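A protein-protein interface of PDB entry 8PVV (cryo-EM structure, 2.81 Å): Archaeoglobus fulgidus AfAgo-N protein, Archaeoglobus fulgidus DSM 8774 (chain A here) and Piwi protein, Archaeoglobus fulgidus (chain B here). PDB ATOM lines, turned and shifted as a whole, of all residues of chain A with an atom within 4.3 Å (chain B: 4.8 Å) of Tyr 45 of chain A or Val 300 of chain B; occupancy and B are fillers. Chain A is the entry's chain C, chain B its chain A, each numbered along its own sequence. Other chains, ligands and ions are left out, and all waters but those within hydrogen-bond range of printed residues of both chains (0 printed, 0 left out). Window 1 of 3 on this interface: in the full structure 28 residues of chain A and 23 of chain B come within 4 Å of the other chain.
Among the printed residues, pairs that only touch across the chains: Tyr 45 of chain A with Val 300 of chain B (3.1 Å), Met 224 of chain A with Phe 308 of chain B (3.2 Å), Leu 44 of chain A with Met 301 of chain B (3.2 Å), Phe 228 of chain A with Trp 299 of chain B (3.2 Å), Ile 46 of chain A with Leu 324 of chain B (3.5 Å), Leu 44 of chain A with Val 300 of chain B (3.6 Å), Asn 47 of chain A with Phe 298 of chain B (3.8 Å), Met 224 of chain A with Met 301 of chain B (3.9 Å), Met 224 of chain A with Trp 299 of chain B (3.9 Å), Leu 44 of chain A with Val 316 of chain B (3.98 Å) and Ile 43 of chain A with Met 301 of chain B (3.997 Å).
The backbone carbonyl oxygen of Ile 46 of chain A lies close to the backbone carbonyl oxygen of Trp 299 of chain B (2.7 Å).
The backbone NH (N) of Trp 299 of chain B sits close to the side-chain amide nitrogen (ND2) of Asn 47 of chain A (3.4 Å).
The backbone carbonyl oxygen (O) of Tyr 45 of chain A sits at hydrogen-bond distance from the backbone NH (N) of Met 301 of chain B (2.9 Å).
O of Tyr 45 of chain A sits close to O of Trp 299 of chain B (3.3 Å).
O of Val 300 of chain B sits close to SD of Met 224 of chain A (3.6 Å).
Of chain B, only Trp 299, Val 300 and Met 301 come within 4 Å of Tyr 45 of chain A.
Of the printed residues of chain B, Leu 44 of chain A touches Val 300 (3.6 Å), Met 301 (3.2 Å) and Val 316 (3.98 Å).
Printed residues of chain A within 4 Å of Met 301 of chain B: Ile 43 (3.997 Å), Leu 44 (3.2 Å), Tyr 45 (2.9 Å) and Met 224 (3.9 Å).
Of the printed residues of chain A, Phe 298 of chain B touches Asn 47.
Printed residues of chain B within 4 Å of Ile 46 of chain A: Trp 299 (2.7 Å) and Leu 324 (3.5 Å).
The nearest residue of chain A that does not touch Val 300 of chain B is Ile 46 of chain A (4.1 Å).
N of Gly 302 of chain B lies within hydrogen-bond range of O of Phe 308 of chain B.
N of Val 316 of chain B sits at hydrogen-bond distance from O of Leu 324 of chain B (2.6 Å).
The backbone NH of Ile 46 of chain A is in hydrogen-bond range of the backbone carbonyl oxygen of Leu 262 of chain A (3.4 Å).
Printed residues of chain B that touch a printed residue of chain A: Phe 298, Trp 299, Val 300, Met 301, Phe 308, Val 316 and Leu 324.
Hydrophobic or aromatic side chains of chain B that line the printed part of chain A: Trp 299, Val 300, Met 301, Phe 308, Val 316 and Leu 324.
Printed residues of chain A that touch a printed residue of chain B: Ile 43, Leu 44, Tyr 45, Ile 46, Asn 47, Met 224 and Phe 228.
Among the printed residues, 16 pairs touch across the chains.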
ATOM      1  N   ILE A  43     -14.605 -20.068  11.372  1.00  0.00           N
ATOM      2  CA  ILE A  43     -13.527 -20.639  10.576  1.00  0.00           C
ATOM      3  C   ILE A  43     -14.065 -20.980   9.195  1.00  0.00           C
ATOM      4  O   ILE A  43     -15.155 -21.547   9.064  1.00  0.00           O
ATOM      5  CB  ILE A  43     -12.922 -21.886  11.253  1.00  0.00           C
ATOM      6  CG1 ILE A  43     -12.279 -21.507  12.585  1.00  0.00           C
ATOM      7  CG2 ILE A  43     -11.909 -22.559  10.343  1.00  0.00           C
ATOM      8  CD1 ILE A  43     -11.135 -20.531  12.446  1.00  0.00           C
ATOM      9  N   LEU A  44     -13.303 -20.621   8.168  1.00  0.00           N
ATOM     10  CA  LEU A  44     -13.650 -20.909   6.786  1.00  0.00           C
ATOM     11  C   LEU A  44     -12.585 -21.807   6.176  1.00  0.00           C
ATOM     12  O   LEU A  44     -11.409 -21.734   6.539  1.00  0.00           O
ATOM     13  CB  LEU A  44     -13.778 -19.623   5.965  1.00  0.00           C
ATOM     14  CG  LEU A  44     -15.144 -18.938   5.884  1.00  0.00           C
ATOM     15  CD1 LEU A  44     -15.681 -18.596   7.264  1.00  0.00           C
ATOM     16  CD2 LEU A  44     -15.044 -17.689   5.032  1.00  0.00           C
ATOM     17  N   TYR A  45     -13.008 -22.657   5.247  1.00  0.00           N
ATOM     18  CA  TYR A  45     -12.122 -23.595   4.574  1.00  0.00           C
ATOM     19  C   TYR A  45     -12.127 -23.302   3.084  1.00  0.00           C
ATOM     20  O   TYR A  45     -13.165 -22.953   2.517  1.00  0.00           O
ATOM     21  CB  TYR A  45     -12.545 -25.037   4.852  1.00  0.00           C
ATOM     22  CG  TYR A  45     -12.600 -25.350   6.326  1.00  0.00           C
ATOM     23  CD1 TYR A  45     -11.459 -25.725   7.018  1.00  0.00           C
ATOM     24  CD2 TYR A  45     -13.788 -25.239   7.032  1.00  0.00           C
ATOM     25  CE1 TYR A  45     -11.503 -26.001   8.369  1.00  0.00           C
ATOM     26  CE2 TYR A  45     -13.843 -25.510   8.381  1.00  0.00           C
ATOM     27  CZ  TYR A  45     -12.698 -25.891   9.046  1.00  0.00           C
ATOM     28  OH  TYR A  45     -12.750 -26.165  10.393  1.00  0.00           O
ATOM     29  N   ILE A  46     -10.969 -23.450   2.452  1.00  0.00           N
ATOM     30  CA  ILE A  46     -10.741 -22.874   1.134  1.00  0.00           C
ATOM     31  C   ILE A  46     -10.595 -23.922   0.035  1.00  0.00           C
ATOM     32  O   ILE A  46     -10.803 -23.584  -1.139  1.00  0.00           O
ATOM     33  CB  ILE A  46      -9.510 -21.941   1.165  1.00  0.00           C
ATOM     34  CG1 ILE A  46      -9.276 -21.266  -0.186  1.00  0.00           C
ATOM     35  CG2 ILE A  46      -8.280 -22.702   1.612  1.00  0.00           C
ATOM     36  CD1 ILE A  46     -10.437 -20.444  -0.644  1.00  0.00           C
ATOM     37  N   ASN A  47     -10.301 -25.177   0.378  1.00  0.00           N
ATOM     38  CA  ASN A  47      -9.990 -26.335  -0.487  1.00  0.00           C
ATOM     39  C   ASN A  47      -8.553 -26.269  -0.986  1.00  0.00           C
ATOM     40  O   ASN A  47      -8.157 -27.086  -1.827  1.00  0.00           O
ATOM     41  CB  ASN A  47     -10.973 -26.546  -1.659  1.00  0.00           C
ATOM     42  CG  ASN A  47     -10.670 -25.701  -2.918  1.00  0.00           C
ATOM     43  OD1 ASN A  47      -9.670 -24.996  -3.020  1.00  0.00           O
ATOM     44  ND2 ASN A  47     -11.563 -25.797  -3.891  1.00  0.00           N
ATOM     45  N   MET A 224     -22.308 -28.730   1.024  1.00  0.00           N
ATOM     46  CA  MET A 224     -20.987 -28.118   0.930  1.00  0.00           C
ATOM     47  C   MET A 224     -19.974 -28.901   1.760  1.00  0.00           C
ATOM     48  O   MET A 224     -18.845 -29.163   1.313  1.00  0.00           O
ATOM     49  CB  MET A 224     -21.074 -26.667   1.402  1.00  0.00           C
ATOM     50  CG  MET A 224     -19.755 -25.949   1.498  1.00  0.00           C
ATOM     51  SD  MET A 224     -19.411 -25.230  -0.117  1.00  0.00           S
ATOM     52  CE  MET A 224     -17.924 -26.088  -0.576  1.00  0.00           C
ATOM     53  N   PHE A 228     -16.592 -30.971   0.460  1.00  0.00           N
ATOM     54  CA  PHE A 228     -15.233 -30.957   1.006  1.00  0.00           C
ATOM     55  C   PHE A 228     -14.782 -32.333   1.481  1.00  0.00           C
ATOM     56  O   PHE A 228     -13.622 -32.716   1.274  1.00  0.00           O
ATOM     57  CB  PHE A 228     -15.099 -29.927   2.125  1.00  0.00           C
ATOM     58  CG  PHE A 228     -14.704 -28.568   1.639  1.00  0.00           C
ATOM     59  CD1 PHE A 228     -13.782 -27.820   2.345  1.00  0.00           C
ATOM     60  CD2 PHE A 228     -15.171 -28.075   0.439  1.00  0.00           C
ATOM     61  CE1 PHE A 228     -13.385 -26.584   1.895  1.00  0.00           C
ATOM     62  CE2 PHE A 228     -14.764 -26.840  -0.018  1.00  0.00           C
ATOM     63  CZ  PHE A 228     -13.877 -26.095   0.713  1.00  0.00           C
ATOM     64  N   PRO A 261      -8.432 -29.325   4.666  1.00  0.00           N
ATOM     65  CA  PRO A 261      -8.701 -27.971   4.177  1.00  0.00           C
ATOM     66  C   PRO A 261      -7.973 -26.931   5.011  1.00  0.00           C
ATOM     67  O   PRO A 261      -7.728 -27.114   6.206  1.00  0.00           O
ATOM     68  CB  PRO A 261     -10.220 -27.838   4.319  1.00  0.00           C
ATOM     69  CG  PRO A 261     -10.572 -28.789   5.407  1.00  0.00           C
ATOM     70  CD  PRO A 261      -9.635 -29.949   5.241  1.00  0.00           C
ATOM     71  N   LEU A 262      -7.624 -25.825   4.362  1.00  0.00           N
ATOM     72  CA  LEU A 262      -6.894 -24.757   5.027  1.00  0.00           C
ATOM     73  C   LEU A 262      -7.869 -23.808   5.710  1.00  0.00           C
ATOM     74  O   LEU A 262      -8.795 -23.294   5.078  1.00  0.00           O
ATOM     75  CB  LEU A 262      -6.030 -24.001   4.023  1.00  0.00           C
ATOM     76  CG  LEU A 262      -5.013 -23.005   4.574  1.00  0.00           C
ATOM     77  CD1 LEU A 262      -4.155 -23.655   5.650  1.00  0.00           C
ATOM     78  CD2 LEU A 262      -4.160 -22.466   3.445  1.00  0.00           C
ATOM     79  N   GLU A 263      -7.654 -23.577   7.001  1.00  0.00           N
ATOM     80  CA  GLU A 263      -8.538 -22.726   7.783  1.00  0.00           C
ATOM     81  C   GLU A 263      -8.323 -21.259   7.438  1.00  0.00           C
ATOM     82  O   GLU A 263      -7.200 -20.829   7.156  1.00  0.00           O
ATOM     83  CB  GLU A 263      -8.302 -22.947   9.276  1.00  0.00           C
ATOM     84  CG  GLU A 263      -8.683 -24.330   9.766  1.00  0.00           C
ATOM     85  CD  GLU A 263      -9.018 -24.351  11.243  1.00  0.00           C
ATOM     86  OE1 GLU A 263      -9.025 -23.268  11.864  1.00  0.00           O
ATOM     87  OE2 GLU A 263      -9.277 -25.447  11.782  1.00  0.00           O
ATOM     88  N   PHE B 298     -11.726 -22.303  -6.593  1.00  0.00           N
ATOM     89  CA  PHE B 298     -11.817 -22.168  -5.146  1.00  0.00           C
ATOM     90  C   PHE B 298     -13.252 -22.333  -4.658  1.00  0.00           C
ATOM     91  O   PHE B 298     -14.198 -21.861  -5.295  1.00  0.00           O
ATOM     92  CB  PHE B 298     -11.268 -20.814  -4.700  1.00  0.00           C
ATOM     93  CG  PHE B 298      -9.867 -20.551  -5.163  1.00  0.00           C
ATOM     94  CD1 PHE B 298      -8.784 -20.987  -4.423  1.00  0.00           C
ATOM     95  CD2 PHE B 298      -9.632 -19.872  -6.344  1.00  0.00           C
ATOM     96  CE1 PHE B 298      -7.495 -20.748  -4.849  1.00  0.00           C
ATOM     97  CE2 PHE B 298      -8.344 -19.631  -6.775  1.00  0.00           C
ATOM     98  CZ  PHE B 298      -7.276 -20.070  -6.026  1.00  0.00           C
ATOM     99  N   TRP B 299     -13.401 -23.010  -3.519  1.00  0.00           N
ATOM    100  CA  TRP B 299     -14.674 -23.197  -2.840  1.00  0.00           C
ATOM    101  C   TRP B 299     -14.481 -22.884  -1.365  1.00  0.00           C
ATOM    102  O   TRP B 299     -13.463 -23.256  -0.779  1.00  0.00           O
ATOM    103  CB  TRP B 299     -15.195 -24.631  -2.997  1.00  0.00           C
ATOM    104  CG  TRP B 299     -15.582 -24.985  -4.388  1.00  0.00           C
ATOM    105  CD1 TRP B 299     -14.778 -25.517  -5.352  1.00  0.00           C
ATOM    106  CD2 TRP B 299     -16.874 -24.836  -4.980  1.00  0.00           C
ATOM    107  NE1 TRP B 299     -15.490 -25.708  -6.510  1.00  0.00           N
ATOM    108  CE2 TRP B 299     -16.780 -25.298  -6.307  1.00  0.00           C
ATOM    109  CE3 TRP B 299     -18.102 -24.356  -4.519  1.00  0.00           C
ATOM    110  CZ2 TRP B 299     -17.865 -25.293  -7.174  1.00  0.00           C
ATOM    111  CZ3 TRP B 299     -19.175 -24.355  -5.381  1.00  0.00           C
ATOM    112  CH2 TRP B 299     -19.052 -24.819  -6.693  1.00  0.00           C
ATOM    113  N   VAL B 300     -15.456 -22.216  -0.757  1.00  0.00           N
ATOM    114  CA  VAL B 300     -15.343 -21.778   0.629  1.00  0.00           C
ATOM    115  C   VAL B 300     -16.452 -22.421   1.449  1.00  0.00           C
ATOM    116  O   VAL B 300     -17.625 -22.376   1.064  1.00  0.00           O
ATOM    117  CB  VAL B 300     -15.385 -20.245   0.753  1.00  0.00           C
ATOM    118  CG1 VAL B 300     -15.002 -19.831   2.156  1.00  0.00           C
ATOM    119  CG2 VAL B 300     -14.447 -19.608  -0.253  1.00  0.00           C
ATOM    120  N   MET B 301     -16.073 -23.016   2.576  1.00  0.00           N
ATOM    121  CA  MET B 301     -16.990 -23.648   3.513  1.00  0.00           C
ATOM    122  C   MET B 301     -17.138 -22.763   4.742  1.00  0.00           C
ATOM    123  O   MET B 301     -16.150 -22.228   5.253  1.00  0.00           O
ATOM    124  CB  MET B 301     -16.482 -25.033   3.920  1.00  0.00           C
ATOM    125  CG  MET B 301     -17.478 -25.871   4.696  1.00  0.00           C
ATOM    126  SD  MET B 301     -16.821 -27.497   5.092  1.00  0.00           S
ATOM    127  CE  MET B 301     -17.475 -27.731   6.739  1.00  0.00           C
ATOM    128  N   GLY B 302     -18.371 -22.608   5.214  1.00  0.00           N
ATOM    129  CA  GLY B 302     -18.625 -21.653   6.273  1.00  0.00           C
ATOM    130  C   GLY B 302     -19.240 -22.208   7.540  1.00  0.00           C
ATOM    131  O   GLY B 302     -18.936 -23.328   7.960  1.00  0.00           O
ATOM    132  N   PHE B 308     -23.354 -24.305   5.952  1.00  0.00           N
ATOM    133  CA  PHE B 308     -21.935 -24.490   5.639  1.00  0.00           C
ATOM    134  C   PHE B 308     -21.475 -23.535   4.542  1.00  0.00           C
ATOM    135  O   PHE B 308     -20.629 -23.872   3.714  1.00  0.00           O
ATOM    136  CB  PHE B 308     -21.636 -25.941   5.258  1.00  0.00           C
ATOM    137  CG  PHE B 308     -21.948 -26.927   6.344  1.00  0.00           C
ATOM    138  CD1 PHE B 308     -20.963 -27.346   7.216  1.00  0.00           C
ATOM    139  CD2 PHE B 308     -23.225 -27.437   6.491  1.00  0.00           C
ATOM    140  CE1 PHE B 308     -21.245 -28.254   8.216  1.00  0.00           C
ATOM    141  CE2 PHE B 308     -23.513 -28.342   7.489  1.00  0.00           C
ATOM    142  CZ  PHE B 308     -22.521 -28.752   8.353  1.00  0.00           C
ATOM    143  N   PRO B 310     -20.357 -19.277   3.677  1.00  0.00           N
ATOM    144  CA  PRO B 310     -19.983 -17.990   4.266  1.00  0.00           C
ATOM    145  C   PRO B 310     -21.115 -16.984   4.158  1.00  0.00           C
ATOM    146  O   PRO B 310     -21.918 -17.009   3.222  1.00  0.00           O
ATOM    147  CB  PRO B 310     -18.774 -17.551   3.430  1.00  0.00           C
ATOM    148  CG  PRO B 310     -18.348 -18.771   2.677  1.00  0.00           C
ATOM    149  CD  PRO B 310     -19.583 -19.564   2.461  1.00  0.00           C
ATOM    150  N   VAL B 316     -12.216 -12.971   1.458  1.00  0.00           N
ATOM    151  CA  VAL B 316     -11.170 -13.911   1.842  1.00  0.00           C
ATOM    152  C   VAL B 316      -9.880 -13.499   1.147  1.00  0.00           C
ATOM    153  O   VAL B 316      -9.831 -13.399  -0.084  1.00  0.00           O
ATOM    154  CB  VAL B 316     -11.558 -15.356   1.487  1.00  0.00           C
ATOM    155  CG1 VAL B 316     -10.321 -16.237   1.401  1.00  0.00           C
ATOM    156  CG2 VAL B 316     -12.542 -15.904   2.508  1.00  0.00           C
ATOM    157  N   LEU B 324     -11.116 -13.305  -2.535  1.00  0.00           N
ATOM    158  CA  LEU B 324     -12.359 -14.026  -2.765  1.00  0.00           C
ATOM    159  C   LEU B 324     -13.483 -13.315  -2.030  1.00  0.00           C
ATOM    160  O   LEU B 324     -13.333 -12.950  -0.861  1.00  0.00           O
ATOM    161  CB  LEU B 324     -12.258 -15.478  -2.308  1.00  0.00           C
ATOM    162  CG  LEU B 324     -11.400 -16.368  -3.203  1.00  0.00           C
ATOM    163  CD1 LEU B 324     -11.395 -17.769  -2.667  1.00  0.00           C
ATOM    164  CD2 LEU B 324     -11.909 -16.350  -4.630  1.00  0.00           C
ATOM    165  N   ILE B 343     -22.082 -22.908  -3.159  1.00  0.00           N
ATOM    166  CA  ILE B 343     -22.007 -21.612  -3.822  1.00  0.00           C
ATOM    167  C   ILE B 343     -20.544 -21.226  -3.974  1.00  0.00           C
ATOM    168  O   ILE B 343     -19.799 -21.186  -2.988  1.00  0.00           O
ATOM    169  CB  ILE B 343     -22.778 -20.540  -3.035  1.00  0.00           C
ATOM    170  CG1 ILE B 343     -24.274 -20.847  -3.047  1.00  0.00           C
ATOM    171  CG2 ILE B 343     -22.519 -19.167  -3.618  1.00  0.00           C
ATOM    172  CD1 ILE B 343     -25.047 -20.130  -1.973  1.00  0.00           C
ATOM    173  N   PRO B 345     -17.560 -18.581  -4.663  1.00  0.00           N
ATOM    174  CA  PRO B 345     -17.370 -17.146  -4.431  1.00  0.00           C
ATOM    175  C   PRO B 345     -16.897 -16.442  -5.699  1.00  0.00           C
ATOM    176  O   PRO B 345     -16.794 -17.031  -6.773  1.00  0.00           O
ATOM    177  CB  PRO B 345     -16.302 -17.113  -3.337  1.00  0.00           C
ATOM    178  CG  PRO B 345     -15.517 -18.352  -3.560  1.00  0.00           C
ATOM    179  CD  PRO B 345     -16.502 -19.387  -4.026  1.00  0.00           C
